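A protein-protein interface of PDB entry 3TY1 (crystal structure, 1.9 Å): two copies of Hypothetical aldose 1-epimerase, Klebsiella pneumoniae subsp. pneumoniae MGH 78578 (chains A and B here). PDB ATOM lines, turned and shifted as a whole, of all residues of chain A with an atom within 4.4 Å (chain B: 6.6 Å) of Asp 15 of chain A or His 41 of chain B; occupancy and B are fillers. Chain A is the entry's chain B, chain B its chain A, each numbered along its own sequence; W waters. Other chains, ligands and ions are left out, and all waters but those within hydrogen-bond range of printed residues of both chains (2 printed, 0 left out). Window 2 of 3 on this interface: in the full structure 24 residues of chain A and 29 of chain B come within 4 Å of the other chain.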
ATOM      1  N   LEU A   7      16.049   6.765 -22.676  1.00  0.00           N
ATOM      2  CA  LEU A   7      16.803   6.060 -23.712  1.00  0.00           C
ATOM      3  C   LEU A   7      17.769   6.965 -24.459  1.00  0.00           C
ATOM      4  O   LEU A   7      18.807   6.496 -24.897  1.00  0.00           O
ATOM      5  CB  LEU A   7      15.850   5.416 -24.734  1.00  0.00           C
ATOM      6  CG  LEU A   7      15.235   4.077 -24.370  1.00  0.00           C
ATOM      7  CD1 LEU A   7      14.871   3.903 -22.908  1.00  0.00           C
ATOM      8  CD2 LEU A   7      14.114   3.764 -25.317  1.00  0.00           C
ATOM      9  N   THR A   8      17.392   8.226 -24.650  1.00  0.00           N
ATOM     10  CA  THR A   8      18.190   9.170 -25.446  1.00  0.00           C
ATOM     11  C   THR A   8      18.027  10.544 -24.801  1.00  0.00           C
ATOM     12  O   THR A   8      16.927  10.930 -24.427  1.00  0.00           O
ATOM     13  CB  THR A   8      17.675   9.239 -26.912  1.00  0.00           C
ATOM     14  OG1 THR A   8      17.676   7.932 -27.453  1.00  0.00           O
ATOM     15  CG2 THR A   8      18.524  10.155 -27.801  1.00  0.00           C
ATOM     16  N   ALA A  10      19.977  14.187 -25.694  1.00  0.00           N
ATOM     17  CA  ALA A  10      21.037  14.920 -26.388  1.00  0.00           C
ATOM     18  C   ALA A  10      21.645  15.991 -25.483  1.00  0.00           C
ATOM     19  O   ALA A  10      22.830  16.258 -25.579  1.00  0.00           O
ATOM     20  CB  ALA A  10      20.527  15.516 -27.671  1.00  0.00           C
ATOM     21  N   GLY A  13      24.213  14.214 -23.995  1.00  0.00           N
ATOM     22  CA  GLY A  13      25.013  13.520 -25.014  1.00  0.00           C
ATOM     23  C   GLY A  13      24.892  12.002 -24.974  1.00  0.00           C
ATOM     24  O   GLY A  13      25.772  11.321 -25.461  1.00  0.00           O
ATOM     25  N   ILE A  14      23.750  11.470 -24.519  1.00  0.00           N
ATOM     26  CA  ILE A  14      23.620  10.022 -24.247  1.00  0.00           C
ATOM     27  C   ILE A  14      22.532   9.332 -25.071  1.00  0.00           C
ATOM     28  O   ILE A  14      21.493   9.944 -25.366  1.00  0.00           O
ATOM     29  CB  ILE A  14      23.402   9.715 -22.716  1.00  0.00           C
ATOM     30  CG1 ILE A  14      21.940   9.793 -22.287  1.00  0.00           C
ATOM     31  CG2 ILE A  14      24.320  10.573 -21.827  1.00  0.00           C
ATOM     32  CD1 ILE A  14      21.240   8.482 -22.336  1.00  0.00           C
ATOM     33  N   ASP A  15      22.810   8.088 -25.471  1.00  0.00           N
ATOM     34  CA  ASP A  15      21.847   7.223 -26.187  1.00  0.00           C
ATOM     35  C   ASP A  15      22.177   5.791 -25.781  1.00  0.00           C
ATOM     36  O   ASP A  15      23.295   5.358 -25.981  1.00  0.00           O
ATOM     37  CB  ASP A  15      21.960   7.338 -27.708  1.00  0.00           C
ATOM     38  CG  ASP A  15      20.689   6.818 -28.450  1.00  0.00           C
ATOM     39  OD1 ASP A  15      19.992   5.888 -27.952  1.00  0.00           O
ATOM     40  OD2 ASP A  15      20.382   7.377 -29.535  1.00  0.00           O
ATOM     41  N   LYS A  16      21.205   5.088 -25.215  1.00  0.00           N
ATOM     42  CA  LYS A  16      21.385   3.708 -24.782  1.00  0.00           C
ATOM     43  C   LYS A  16      21.547   2.707 -25.926  1.00  0.00           C
ATOM     44  O   LYS A  16      22.053   1.628 -25.689  1.00  0.00           O
ATOM     45  CB  LYS A  16      20.233   3.258 -23.860  1.00  0.00           C
ATOM     46  CG  LYS A  16      20.316   3.801 -22.432  1.00  0.00           C
ATOM     47  CD  LYS A  16      19.092   3.369 -21.633  1.00  0.00           C
ATOM     48  CE  LYS A  16      19.026   4.010 -20.248  1.00  0.00           C
ATOM     49  NZ  LYS A  16      19.751   3.209 -19.259  1.00  0.00           N
ATOM     50  N   GLY A  17      21.110   3.031 -27.138  1.00  0.00           N
ATOM     51  CA  GLY A  17      21.175   2.067 -28.248  1.00  0.00           C
ATOM     52  C   GLY A  17      20.311   0.829 -27.948  1.00  0.00           C
ATOM     53  O   GLY A  17      19.118   0.952 -27.606  1.00  0.00           O
ATOM     54  N   GLN A  37      14.439  -1.375 -27.724  1.00  0.00           N
ATOM     55  CA  GLN A  37      15.082  -0.510 -28.702  1.00  0.00           C
ATOM     56  C   GLN A  37      16.153  -1.352 -29.381  1.00  0.00           C
ATOM     57  O   GLN A  37      16.913  -2.070 -28.713  1.00  0.00           O
ATOM     58  CB  GLN A  37      15.702   0.730 -28.073  1.00  0.00           C
ATOM     59  CG  GLN A  37      16.195   1.728 -29.149  1.00  0.00           C
ATOM     60  CD  GLN A  37      16.458   3.087 -28.639  1.00  0.00           C
ATOM     61  OE1 GLN A  37      15.638   3.999 -28.830  1.00  0.00           O
ATOM     62  NE2 GLN A  37      17.606   3.268 -28.005  1.00  0.00           N
ATOM     63  N   LYS A  49      17.296   3.530 -35.543  1.00  0.00           N
ATOM     64  CA  LYS A  49      16.768   2.815 -34.395  1.00  0.00           C
ATOM     65  C   LYS A  49      15.302   2.539 -34.584  1.00  0.00           C
ATOM     66  O   LYS A  49      14.595   3.364 -35.162  1.00  0.00           O
ATOM     67  CB  LYS A  49      16.902   3.672 -33.151  1.00  0.00           C
ATOM     68  CG  LYS A  49      18.340   3.950 -32.732  1.00  0.00           C
ATOM     69  CD  LYS A  49      18.423   4.916 -31.558  1.00  0.00           C
ATOM     70  CE  LYS A  49      18.174   6.400 -32.001  1.00  0.00           C
ATOM     71  NZ  LYS A  49      18.062   7.377 -30.877  1.00  0.00           N
ATOM     72  N   ASN B  18      36.149   8.200 -27.762  1.00  0.00           N
ATOM     73  CA  ASN B  18      36.308   8.667 -26.380  1.00  0.00           C
ATOM     74  C   ASN B  18      37.745   8.494 -25.886  1.00  0.00           C
ATOM     75  O   ASN B  18      38.306   7.428 -26.025  1.00  0.00           O
ATOM     76  CB  ASN B  18      35.339   7.967 -25.440  1.00  0.00           C
ATOM     77  CG  ASN B  18      33.886   8.316 -25.729  1.00  0.00           C
ATOM     78  OD1 ASN B  18      33.516   9.472 -25.915  1.00  0.00           O
ATOM     79  ND2 ASN B  18      33.057   7.299 -25.771  1.00  0.00           N
ATOM     80  N   VAL B  39      32.493  11.460 -27.703  1.00  0.00           N
ATOM     81  CA  VAL B  39      31.604  11.200 -28.809  1.00  0.00           C
ATOM     82  C   VAL B  39      30.221  11.445 -28.276  1.00  0.00           C
ATOM     83  O   VAL B  39      29.820  10.829 -27.284  1.00  0.00           O
ATOM     84  CB  VAL B  39      31.696   9.749 -29.336  1.00  0.00           C
ATOM     85  CG1 VAL B  39      30.768   9.567 -30.578  1.00  0.00           C
ATOM     86  CG2 VAL B  39      33.104   9.404 -29.723  1.00  0.00           C
ATOM     87  N   LEU B  40      29.483  12.329 -28.923  1.00  0.00           N
ATOM     88  CA  LEU B  40      28.139  12.710 -28.470  1.00  0.00           C
ATOM     89  C   LEU B  40      27.047  11.871 -29.148  1.00  0.00           C
ATOM     90  O   LEU B  40      27.246  11.240 -30.191  1.00  0.00           O
ATOM     91  CB  LEU B  40      27.876  14.203 -28.704  1.00  0.00           C
ATOM     92  CG  LEU B  40      28.828  15.166 -28.007  1.00  0.00           C
ATOM     93  CD1 LEU B  40      28.483  16.589 -28.550  1.00  0.00           C
ATOM     94  CD2 LEU B  40      28.723  15.016 -26.493  1.00  0.00           C
ATOM     95  N   HIS B  41      25.856  11.910 -28.552  1.00  0.00           N
ATOM     96  CA  HIS B  41      24.725  11.104 -29.008  1.00  0.00           C
ATOM     97  C   HIS B  41      23.429  11.891 -28.828  1.00  0.00           C
ATOM     98  O   HIS B  41      23.374  12.876 -28.065  1.00  0.00           O
ATOM     99  CB  HIS B  41      24.652   9.757 -28.281  1.00  0.00           C
ATOM    100  CG  HIS B  41      25.876   8.912 -28.427  1.00  0.00           C
ATOM    101  ND1 HIS B  41      26.143   8.176 -29.565  1.00  0.00           N
ATOM    102  CD2 HIS B  41      26.917   8.689 -27.575  1.00  0.00           C
ATOM    103  CE1 HIS B  41      27.298   7.543 -29.412  1.00  0.00           C
ATOM    104  NE2 HIS B  41      27.778   7.824 -28.212  1.00  0.00           N
ATOM    105  N   GLY B  42      22.397  11.466 -29.546  1.00  0.00           N
ATOM    106  CA  GLY B  42      21.070  12.055 -29.444  1.00  0.00           C
ATOM    107  C   GLY B  42      20.774  13.091 -30.515  1.00  0.00           C
ATOM    108  O   GLY B  42      21.654  13.872 -30.920  1.00  0.00           O
ATOM    109  N   GLY B  43      19.531  13.100 -31.000  1.00  0.00           N
ATOM    110  CA  GLY B  43      19.149  14.098 -31.989  1.00  0.00           C
ATOM    111  C   GLY B  43      20.056  14.123 -33.213  1.00  0.00           C
ATOM    112  O   GLY B  43      20.515  13.089 -33.660  1.00  0.00           O
ATOM    113  N   GLN B  45      22.955  15.274 -33.250  1.00  0.00           N
ATOM    114  CA  GLN B  45      24.293  15.301 -32.670  1.00  0.00           C
ATOM    115  C   GLN B  45      24.907  13.902 -32.662  1.00  0.00           C
ATOM    116  O   GLN B  45      26.037  13.714 -32.228  1.00  0.00           O
ATOM    117  CB  GLN B  45      24.124  16.015 -31.292  1.00  0.00           C
ATOM    118  CG  GLN B  45      24.988  15.738 -30.246  1.00  0.00           C
ATOM    119  CD  GLN B  45      24.637  16.499 -29.022  1.00  0.00           C
ATOM    120  OE1 GLN B  45      24.778  17.731 -28.985  1.00  0.00           O
ATOM    121  NE2 GLN B  45      24.320  15.779 -27.965  1.00  0.00           N
ATOM    122  N   GLU B  46      24.187  12.900 -33.197  1.00  0.00           N
ATOM    123  CA  GLU B  46      24.666  11.526 -33.185  1.00  0.00           C
ATOM    124  C   GLU B  46      26.012  11.381 -33.910  1.00  0.00           C
ATOM    125  O   GLU B  46      26.125  11.733 -35.062  1.00  0.00           O
ATOM    126  CB  GLU B  46      23.663  10.560 -33.814  1.00  0.00           C
ATOM    127  CG  GLU B  46      24.145   9.079 -33.801  1.00  0.00           C
ATOM    128  CD  GLU B  46      24.548   8.542 -32.390  1.00  0.00           C
ATOM    129  OE1 GLU B  46      23.784   8.737 -31.437  1.00  0.00           O
ATOM    130  OE2 GLU B  46      25.600   7.901 -32.249  1.00  0.00           O
ATOM    131  N   GLY B  47      27.023  10.932 -33.185  1.00  0.00           N
ATOM    132  CA  GLY B  47      28.357  10.724 -33.753  1.00  0.00           C
ATOM    133  C   GLY B  47      29.268  11.941 -33.731  1.00  0.00           C
ATOM    134  O   GLY B  47      30.425  11.802 -34.024  1.00  0.00           O
ATOM    135  N   SER B  48      28.758  13.125 -33.374  1.00  0.00           N
ATOM    136  CA  SER B  48      29.564  14.327 -33.304  1.00  0.00           C
ATOM    137  C   SER B  48      30.563  14.244 -32.179  1.00  0.00           C
ATOM    138  O   SER B  48      30.239  13.743 -31.118  1.00  0.00           O
ATOM    139  CB  SER B  48      28.706  15.561 -33.056  1.00  0.00           C
ATOM    140  OG  SER B  48      27.919  15.864 -34.204  1.00  0.00           O
HETATM  141  O   HOH W   1      28.278  11.479 -24.852  1.00  0.00           O
HETATM  142  O   HOH W   2      21.448   9.235 -31.050  1.00  0.00           O
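NE2 of Gln 45 of chain B sits at hydrogen-bond distance from O of Ala 10 of chain A, at 2.9 Å. The backbone NH (N) of His 41 of chain B lies within hydrogen-bond range of the backbone carbonyl oxygen (O) of Gly 13 of chain A (3.1 Å).
A ring nitrogen (ND1) of His 41 of chain B is in hydrogen-bond range of the side-chain carboxylate (OE2) of Glu 46 of chain B (2.8 Å). N of Gly 17 of chain A sits at hydrogen-bond distance from OD1 of Asp 15 of chain A, 3.2 Å away. N of Leu 40 of chain B is in hydrogen-bond range of O of Ser 48 of chain B (2.7 Å). The side-chain hydroxyl of Thr 8 of chain A sits at hydrogen-bond distance from the side-chain carboxylate of Asp 15 of chain A, 3.1 Å away. The backbone carbonyl oxygen (O) of Leu 40 of chain B lies within hydrogen-bond range of the backbone NH (N) of Gly 47 of chain B, at 3.0 Å. OD2 of Asp 15 of chain A lies within salt-bridge range of NZ of Lys 49 of chain A (2.7 Å).
Thr 8 of chain A touches Gly 42 of chain B. Ala 10 of chain A touches His 41 of chain B (CA to O, 3.5 Å). Ala 10 of chain A touches Gly 42 of chain B. C of Leu 40 of chain B touches O of Gly 13 of chain A (3.9 Å). Gln 45 of chain B touches Gly 13 of chain A. Ile 14 of chain A touches His 41 of chain B. CB of His 41 of chain B touches CB of Asp 15 of chain A (3.7 Å).
Of the printed residues of chain B, Thr 8 of chain A touches Gly 42. Of the printed residues of chain B, Ala 10 of chain A touches His 41 (3.5 Å), Gly 42 (3.7 Å) and Gln 45 (2.9 Å). Asp 15 of chain A touches just one residue of chain B: His 41. Of the printed residues of chain A, His 41 of chain B touches Ala 10 (3.5 Å), Gly 13 (3.1 Å), Ile 14 (3.8 Å) and Asp 15 (3.7 Å). Of the printed residues of chain A, Gly 42 of chain B touches Thr 8 (3.6 Å) and Ala 10 (3.7 Å).
Printed residues of chain A that touch a printed residue of chain B: Thr 8, Ala 10, Gly 13, Ile 14 and Asp 15. Among the printed residues, 9 pairs touch across the chains. Among the printed residues, no Asp or Glu carboxylate lies within 4 Å of a Lys or Arg side-chain nitrogen of the other chain.
No position is printed for both chains. Of the 9 pairs that touch across the chains among the printed residues, none has its exchanged pair printed and touching as well.
Water W2 lies within hydrogen-bond range of OE1 of Glu 46 of chain B, OD2 of Asp 15 of chain A and N of Gly 42 of chain B. Water W1 bridges the backbone carbonyl oxygen (O) of Gly 13 of chain A (2.6 Å) and the backbone carbonyl oxygen (O) of Val 39 of chain B (3.0 Å).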
